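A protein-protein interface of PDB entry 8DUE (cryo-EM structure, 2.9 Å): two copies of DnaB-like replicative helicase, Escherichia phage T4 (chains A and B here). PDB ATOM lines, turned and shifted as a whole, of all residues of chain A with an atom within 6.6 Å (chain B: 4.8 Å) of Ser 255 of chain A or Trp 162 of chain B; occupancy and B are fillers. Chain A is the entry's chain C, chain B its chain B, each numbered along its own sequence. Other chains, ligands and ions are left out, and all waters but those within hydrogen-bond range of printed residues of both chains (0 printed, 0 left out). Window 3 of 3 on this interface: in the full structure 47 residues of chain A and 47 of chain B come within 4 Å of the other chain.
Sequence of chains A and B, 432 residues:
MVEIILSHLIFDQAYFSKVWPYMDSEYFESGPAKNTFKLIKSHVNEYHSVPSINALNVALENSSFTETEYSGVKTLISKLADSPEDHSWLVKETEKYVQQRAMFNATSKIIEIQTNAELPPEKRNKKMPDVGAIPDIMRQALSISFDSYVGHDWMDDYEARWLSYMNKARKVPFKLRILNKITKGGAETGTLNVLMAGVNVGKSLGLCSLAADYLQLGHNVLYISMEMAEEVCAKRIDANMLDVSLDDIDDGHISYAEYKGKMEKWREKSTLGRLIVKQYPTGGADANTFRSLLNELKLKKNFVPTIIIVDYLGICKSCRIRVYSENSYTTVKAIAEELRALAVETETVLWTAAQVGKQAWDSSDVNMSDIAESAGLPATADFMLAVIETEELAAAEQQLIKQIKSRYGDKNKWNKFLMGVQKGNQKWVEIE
The side-chain hydroxyl (OH) of Tyr 158 of chain B lies close to the side-chain amino group (NZ) of Lys 260 of chain A (3.3 Å).
OH of Tyr 256 of chain A sits at hydrogen-bond distance from OE2 of Glu 159 of chain B, at 2.5 Å.
The side-chain amino group (NZ) of Lys 260 of chain A is in salt-bridge range of the side-chain carboxylate (OE2) of Glu 159 of chain B, 3.0 Å away.
The guanidinium group (NH1) of Arg 161 of chain B lies within hydrogen-bond range of the side-chain hydroxyl (OH) of Tyr 259 of chain A (3.0 Å).
NH1 of Arg 161 of chain B lies within hydrogen-bond range of OH of Tyr 165 of chain B (3.1 Å).
The backbone carbonyl oxygen (O) of Asp 248 of chain A is in hydrogen-bond range of the backbone NH (N) of Ile 254 of chain A, at 3.2 Å.
The side-chain hydroxyl (OG) of Ser 255 of chain A lies close to the backbone NH (N) of Glu 258 of chain A, 3.4 Å away.
The side-chain amino group (NZ) of Lys 260 of chain A sits close to the side-chain hydroxyl (OH) of Tyr 256 of chain A, at 3.5 Å.
Among the printed residues, merely in contact across the chains: Ile 254 of chain A with Trp 162 of chain B (3.1 Å), Ser 255 of chain A with Trp 162 of chain B (3.9 Å), Tyr 256 of chain A with Trp 162 of chain B (3.2 Å), Tyr 259 of chain A with Trp 162 of chain B (3.9 Å) and Tyr 259 of chain A with Tyr 165 of chain B (3.4 Å).
Ser 255 of chain A touches one residue of chain B.
Trp 162 of chain B touches four residues of chain A.
Printed residues of chain B within 4 Å of Ile 254 of chain A: Trp 162 (3.1 Å).
Of the printed residues of chain A, Tyr 165 of chain B touches Tyr 259.
Of the 9 printed residues of chain B, 5 touch a printed residue of chain A.
No position is printed for both chains.
Of the 9 pairs that touch across the chains among the printed residues, none has its exchanged pair printed and touching as well.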
ATOM      1  N   ASP A 248       4.920  28.902   6.567  1.00  0.00           N
ATOM      2  CA  ASP A 248       5.287  29.295   7.921  1.00  0.00           C
ATOM      3  C   ASP A 248       4.966  28.210   8.939  1.00  0.00           C
ATOM      4  O   ASP A 248       5.553  28.194  10.026  1.00  0.00           O
ATOM      5  CB  ASP A 248       4.582  30.598   8.291  1.00  0.00           C
ATOM      6  CG  ASP A 248       4.810  31.693   7.267  1.00  0.00           C
ATOM      7  OD1 ASP A 248       5.411  31.402   6.212  1.00  0.00           O
ATOM      8  OD2 ASP A 248       4.388  32.842   7.516  1.00  0.00           O
ATOM      9  N   ILE A 249       4.046  27.301   8.617  1.00  0.00           N
ATOM     10  CA  ILE A 249       3.687  26.260   9.574  1.00  0.00           C
ATOM     11  C   ILE A 249       4.823  25.257   9.731  1.00  0.00           C
ATOM     12  O   ILE A 249       5.178  24.873  10.853  1.00  0.00           O
ATOM     13  CB  ILE A 249       2.376  25.574   9.154  1.00  0.00           C
ATOM     14  CG1 ILE A 249       1.233  26.588   9.144  1.00  0.00           C
ATOM     15  CG2 ILE A 249       2.054  24.422  10.092  1.00  0.00           C
ATOM     16  CD1 ILE A 249      -0.117  25.975   8.892  1.00  0.00           C
ATOM     17  N   GLY A 252       8.740  26.806  10.789  1.00  0.00           N
ATOM     18  CA  GLY A 252       9.001  27.277  12.132  1.00  0.00           C
ATOM     19  C   GLY A 252       8.724  28.742  12.372  1.00  0.00           C
ATOM     20  O   GLY A 252       8.968  29.225  13.483  1.00  0.00           O
ATOM     21  N   HIS A 253       8.225  29.471  11.369  1.00  0.00           N
ATOM     22  CA  HIS A 253       7.882  30.873  11.581  1.00  0.00           C
ATOM     23  C   HIS A 253       6.746  31.027  12.583  1.00  0.00           C
ATOM     24  O   HIS A 253       6.673  32.044  13.283  1.00  0.00           O
ATOM     25  CB  HIS A 253       7.513  31.535  10.253  1.00  0.00           C
ATOM     26  CG  HIS A 253       8.663  31.672   9.304  1.00  0.00           C
ATOM     27  ND1 HIS A 253       8.743  32.685   8.373  1.00  0.00           N
ATOM     28  CD2 HIS A 253       9.780  30.923   9.140  1.00  0.00           C
ATOM     29  CE1 HIS A 253       9.858  32.557   7.678  1.00  0.00           C
ATOM     30  NE2 HIS A 253      10.506  31.495   8.123  1.00  0.00           N
ATOM     31  N   ILE A 254       5.861  30.042  12.667  1.00  0.00           N
ATOM     32  CA  ILE A 254       4.800  30.052  13.666  1.00  0.00           C
ATOM     33  C   ILE A 254       5.394  29.660  15.012  1.00  0.00           C
ATOM     34  O   ILE A 254       6.114  28.660  15.124  1.00  0.00           O
ATOM     35  CB  ILE A 254       3.651  29.116  13.254  1.00  0.00           C
ATOM     36  CG1 ILE A 254       2.565  29.073  14.332  1.00  0.00           C
ATOM     37  CG2 ILE A 254       4.165  27.717  12.938  1.00  0.00           C
ATOM     38  CD1 ILE A 254       1.765  30.352  14.446  1.00  0.00           C
ATOM     39  N   SER A 255       5.127  30.466  16.031  1.00  0.00           N
ATOM     40  CA  SER A 255       5.616  30.214  17.376  1.00  0.00           C
ATOM     41  C   SER A 255       4.510  29.614  18.234  1.00  0.00           C
ATOM     42  O   SER A 255       3.321  29.825  17.992  1.00  0.00           O
ATOM     43  CB  SER A 255       6.135  31.502  18.015  1.00  0.00           C
ATOM     44  OG  SER A 255       5.099  32.461  18.128  1.00  0.00           O
ATOM     45  N   TYR A 256       4.921  28.846  19.247  1.00  0.00           N
ATOM     46  CA  TYR A 256       3.943  28.218  20.128  1.00  0.00           C
ATOM     47  C   TYR A 256       3.119  29.254  20.878  1.00  0.00           C
ATOM     48  O   TYR A 256       1.961  28.994  21.217  1.00  0.00           O
ATOM     49  CB  TYR A 256       4.635  27.282  21.118  1.00  0.00           C
ATOM     50  CG  TYR A 256       3.689  26.677  22.132  1.00  0.00           C
ATOM     51  CD1 TYR A 256       2.750  25.730  21.754  1.00  0.00           C
ATOM     52  CD2 TYR A 256       3.733  27.056  23.465  1.00  0.00           C
ATOM     53  CE1 TYR A 256       1.884  25.173  22.674  1.00  0.00           C
ATOM     54  CE2 TYR A 256       2.870  26.505  24.393  1.00  0.00           C
ATOM     55  CZ  TYR A 256       1.947  25.564  23.992  1.00  0.00           C
ATOM     56  OH  TYR A 256       1.086  25.013  24.912  1.00  0.00           O
ATOM     57  N   ALA A 257       3.692  30.429  21.143  1.00  0.00           N
ATOM     58  CA  ALA A 257       2.930  31.489  21.792  1.00  0.00           C
ATOM     59  C   ALA A 257       1.772  31.947  20.914  1.00  0.00           C
ATOM     60  O   ALA A 257       0.619  31.989  21.358  1.00  0.00           O
ATOM     61  CB  ALA A 257       3.848  32.664  22.132  1.00  0.00           C
ATOM     62  N   GLU A 258       2.062  32.286  19.655  1.00  0.00           N
ATOM     63  CA  GLU A 258       1.009  32.724  18.742  1.00  0.00           C
ATOM     64  C   GLU A 258       0.006  31.608  18.478  1.00  0.00           C
ATOM     65  O   GLU A 258      -1.205  31.854  18.413  1.00  0.00           O
ATOM     66  CB  GLU A 258       1.616  33.211  17.427  1.00  0.00           C
ATOM     67  CG  GLU A 258       2.531  34.412  17.562  1.00  0.00           C
ATOM     68  CD  GLU A 258       3.005  34.927  16.218  1.00  0.00           C
ATOM     69  OE1 GLU A 258       2.433  34.508  15.189  1.00  0.00           O
ATOM     70  OE2 GLU A 258       3.946  35.747  16.189  1.00  0.00           O
ATOM     71  N   TYR A 259       0.494  30.378  18.306  1.00  0.00           N
ATOM     72  CA  TYR A 259      -0.399  29.256  18.043  1.00  0.00           C
ATOM     73  C   TYR A 259      -1.345  29.029  19.214  1.00  0.00           C
ATOM     74  O   TYR A 259      -2.555  28.866  19.028  1.00  0.00           O
ATOM     75  CB  TYR A 259       0.422  28.000  17.754  1.00  0.00           C
ATOM     76  CG  TYR A 259      -0.335  26.904  17.043  1.00  0.00           C
ATOM     77  CD1 TYR A 259      -0.404  26.870  15.657  1.00  0.00           C
ATOM     78  CD2 TYR A 259      -0.971  25.897  17.755  1.00  0.00           C
ATOM     79  CE1 TYR A 259      -1.089  25.869  15.003  1.00  0.00           C
ATOM     80  CE2 TYR A 259      -1.659  24.893  17.109  1.00  0.00           C
ATOM     81  CZ  TYR A 259      -1.715  24.884  15.733  1.00  0.00           C
ATOM     82  OH  TYR A 259      -2.400  23.885  15.087  1.00  0.00           O
ATOM     83  N   LYS A 260      -0.807  29.038  20.436  1.00  0.00           N
ATOM     84  CA  LYS A 260      -1.640  28.873  21.622  1.00  0.00           C
ATOM     85  C   LYS A 260      -2.635  30.017  21.759  1.00  0.00           C
ATOM     86  O   LYS A 260      -3.809  29.795  22.083  1.00  0.00           O
ATOM     87  CB  LYS A 260      -0.753  28.782  22.865  1.00  0.00           C
ATOM     88  CG  LYS A 260      -1.502  28.578  24.169  1.00  0.00           C
ATOM     89  CD  LYS A 260      -1.509  27.116  24.577  1.00  0.00           C
ATOM     90  CE  LYS A 260      -2.083  26.934  25.973  1.00  0.00           C
ATOM     91  NZ  LYS A 260      -1.991  25.520  26.425  1.00  0.00           N
ATOM     92  N   TYR B 158      -4.811  19.709  20.259  1.00  0.00           N
ATOM     93  CA  TYR B 158      -3.939  20.543  19.438  1.00  0.00           C
ATOM     94  C   TYR B 158      -2.517  20.614  19.980  1.00  0.00           C
ATOM     95  O   TYR B 158      -1.599  20.964  19.229  1.00  0.00           O
ATOM     96  CB  TYR B 158      -4.524  21.951  19.300  1.00  0.00           C
ATOM     97  CG  TYR B 158      -4.387  22.829  20.524  1.00  0.00           C
ATOM     98  CD1 TYR B 158      -5.251  22.695  21.601  1.00  0.00           C
ATOM     99  CD2 TYR B 158      -3.410  23.812  20.590  1.00  0.00           C
ATOM    100  CE1 TYR B 158      -5.135  23.503  22.715  1.00  0.00           C
ATOM    101  CE2 TYR B 158      -3.287  24.625  21.700  1.00  0.00           C
ATOM    102  CZ  TYR B 158      -4.151  24.466  22.759  1.00  0.00           C
ATOM    103  OH  TYR B 158      -4.034  25.271  23.868  1.00  0.00           O
ATOM    104  N   GLU B 159      -2.309  20.291  21.259  1.00  0.00           N
ATOM    105  CA  GLU B 159      -0.951  20.257  21.793  1.00  0.00           C
ATOM    106  C   GLU B 159      -0.118  19.180  21.111  1.00  0.00           C
ATOM    107  O   GLU B 159       1.044  19.411  20.762  1.00  0.00           O
ATOM    108  CB  GLU B 159      -0.982  20.037  23.306  1.00  0.00           C
ATOM    109  CG  GLU B 159      -1.469  21.237  24.106  1.00  0.00           C
ATOM    110  CD  GLU B 159      -0.457  22.370  24.151  1.00  0.00           C
ATOM    111  OE1 GLU B 159       0.704  22.158  23.744  1.00  0.00           O
ATOM    112  OE2 GLU B 159      -0.824  23.477  24.598  1.00  0.00           O
ATOM    113  N   ALA B 160      -0.698  17.994  20.910  1.00  0.00           N
ATOM    114  CA  ALA B 160       0.016  16.934  20.206  1.00  0.00           C
ATOM    115  C   ALA B 160       0.297  17.327  18.762  1.00  0.00           C
ATOM    116  O   ALA B 160       1.365  17.015  18.220  1.00  0.00           O
ATOM    117  CB  ALA B 160      -0.784  15.633  20.267  1.00  0.00           C
ATOM    118  N   ARG B 161      -0.653  18.007  18.121  1.00  0.00           N
ATOM    119  CA  ARG B 161      -0.436  18.468  16.754  1.00  0.00           C
ATOM    120  C   ARG B 161       0.704  19.475  16.687  1.00  0.00           C
ATOM    121  O   ARG B 161       1.514  19.447  15.754  1.00  0.00           O
ATOM    122  CB  ARG B 161      -1.726  19.065  16.191  1.00  0.00           C
ATOM    123  CG  ARG B 161      -2.940  18.151  16.334  1.00  0.00           C
ATOM    124  CD  ARG B 161      -4.155  18.675  15.581  1.00  0.00           C
ATOM    125  NE  ARG B 161      -4.609  19.971  16.071  1.00  0.00           N
ATOM    126  CZ  ARG B 161      -4.305  21.130  15.505  1.00  0.00           C
ATOM    127  NH1 ARG B 161      -3.532  21.192  14.434  1.00  0.00           N
ATOM    128  NH2 ARG B 161      -4.787  22.254  16.027  1.00  0.00           N
ATOM    129  N   TRP B 162       0.793  20.372  17.672  1.00  0.00           N
ATOM    130  CA  TRP B 162       1.920  21.298  17.692  1.00  0.00           C
ATOM    131  C   TRP B 162       3.230  20.584  17.993  1.00  0.00           C
ATOM    132  O   TRP B 162       4.280  20.984  17.481  1.00  0.00           O
ATOM    133  CB  TRP B 162       1.698  22.416  18.706  1.00  0.00           C
ATOM    134  CG  TRP B 162       2.886  23.320  18.789  1.00  0.00           C
ATOM    135  CD1 TRP B 162       3.803  23.376  19.794  1.00  0.00           C
ATOM    136  CD2 TRP B 162       3.313  24.266  17.801  1.00  0.00           C
ATOM    137  NE1 TRP B 162       4.762  24.317  19.508  1.00  0.00           N
ATOM    138  CE2 TRP B 162       4.485  24.877  18.288  1.00  0.00           C
ATOM    139  CE3 TRP B 162       2.812  24.664  16.559  1.00  0.00           C
ATOM    140  CZ2 TRP B 162       5.163  25.862  17.575  1.00  0.00           C
ATOM    141  CZ3 TRP B 162       3.487  25.642  15.854  1.00  0.00           C
ATOM    142  CH2 TRP B 162       4.649  26.231  16.364  1.00  0.00           C
ATOM    143  N   LEU B 163       3.198  19.547  18.832  1.00  0.00           N
ATOM    144  CA  LEU B 163       4.390  18.729  19.034  1.00  0.00           C
ATOM    145  C   LEU B 163       4.853  18.128  17.716  1.00  0.00           C
ATOM    146  O   LEU B 163       6.051  18.104  17.412  1.00  0.00           O
ATOM    147  CB  LEU B 163       4.108  17.628  20.056  1.00  0.00           C
ATOM    148  CG  LEU B 163       3.805  18.055  21.491  1.00  0.00           C
ATOM    149  CD1 LEU B 163       3.496  16.841  22.349  1.00  0.00           C
ATOM    150  CD2 LEU B 163       4.962  18.847  22.073  1.00  0.00           C
ATOM    151  N   SER B 164       3.904  17.637  16.917  1.00  0.00           N
ATOM    152  CA  SER B 164       4.242  17.103  15.602  1.00  0.00           C
ATOM    153  C   SER B 164       4.808  18.181  14.687  1.00  0.00           C
ATOM    154  O   SER B 164       5.760  17.923  13.941  1.00  0.00           O
ATOM    155  CB  SER B 164       3.011  16.456  14.969  1.00  0.00           C
ATOM    156  OG  SER B 164       2.524  15.401  15.778  1.00  0.00           O
ATOM    157  N   TYR B 165       4.236  19.386  14.719  1.00  0.00           N
ATOM    158  CA  TYR B 165       4.757  20.479  13.899  1.00  0.00           C
ATOM    159  C   TYR B 165       6.185  20.833  14.295  1.00  0.00           C
ATOM    160  O   TYR B 165       7.047  21.045  13.435  1.00  0.00           O
ATOM    161  CB  TYR B 165       3.865  21.714  14.029  1.00  0.00           C
ATOM    162  CG  TYR B 165       2.455  21.548  13.523  1.00  0.00           C
ATOM    163  CD1 TYR B 165       2.186  20.846  12.357  1.00  0.00           C
ATOM    164  CD2 TYR B 165       1.389  22.097  14.217  1.00  0.00           C
ATOM    165  CE1 TYR B 165       0.891  20.699  11.900  1.00  0.00           C
ATOM    166  CE2 TYR B 165       0.094  21.952  13.771  1.00  0.00           C
ATOM    167  CZ  TYR B 165      -0.148  21.253  12.613  1.00  0.00           C
ATOM    168  OH  TYR B 165      -1.437  21.112  12.170  1.00  0.00           O
ATOM    169  N   MET B 166       6.449  20.911  15.600  1.00  0.00           N
ATOM    170  CA  MET B 166       7.752  21.348  16.087  1.00  0.00           C
ATOM    171  C   MET B 166       8.822  20.284  15.878  1.00  0.00           C
ATOM    172  O   MET B 166       9.927  20.594  15.419  1.00  0.00           O
ATOM    173  CB  MET B 166       7.646  21.725  17.566  1.00  0.00           C
ATOM    174  CG  MET B 166       8.936  21.591  18.352  1.00  0.00           C
ATOM    175  SD  MET B 166       8.720  22.097  20.069  1.00  0.00           S
ATOM    176  CE  MET B 166       7.196  21.247  20.474  1.00  0.00           C
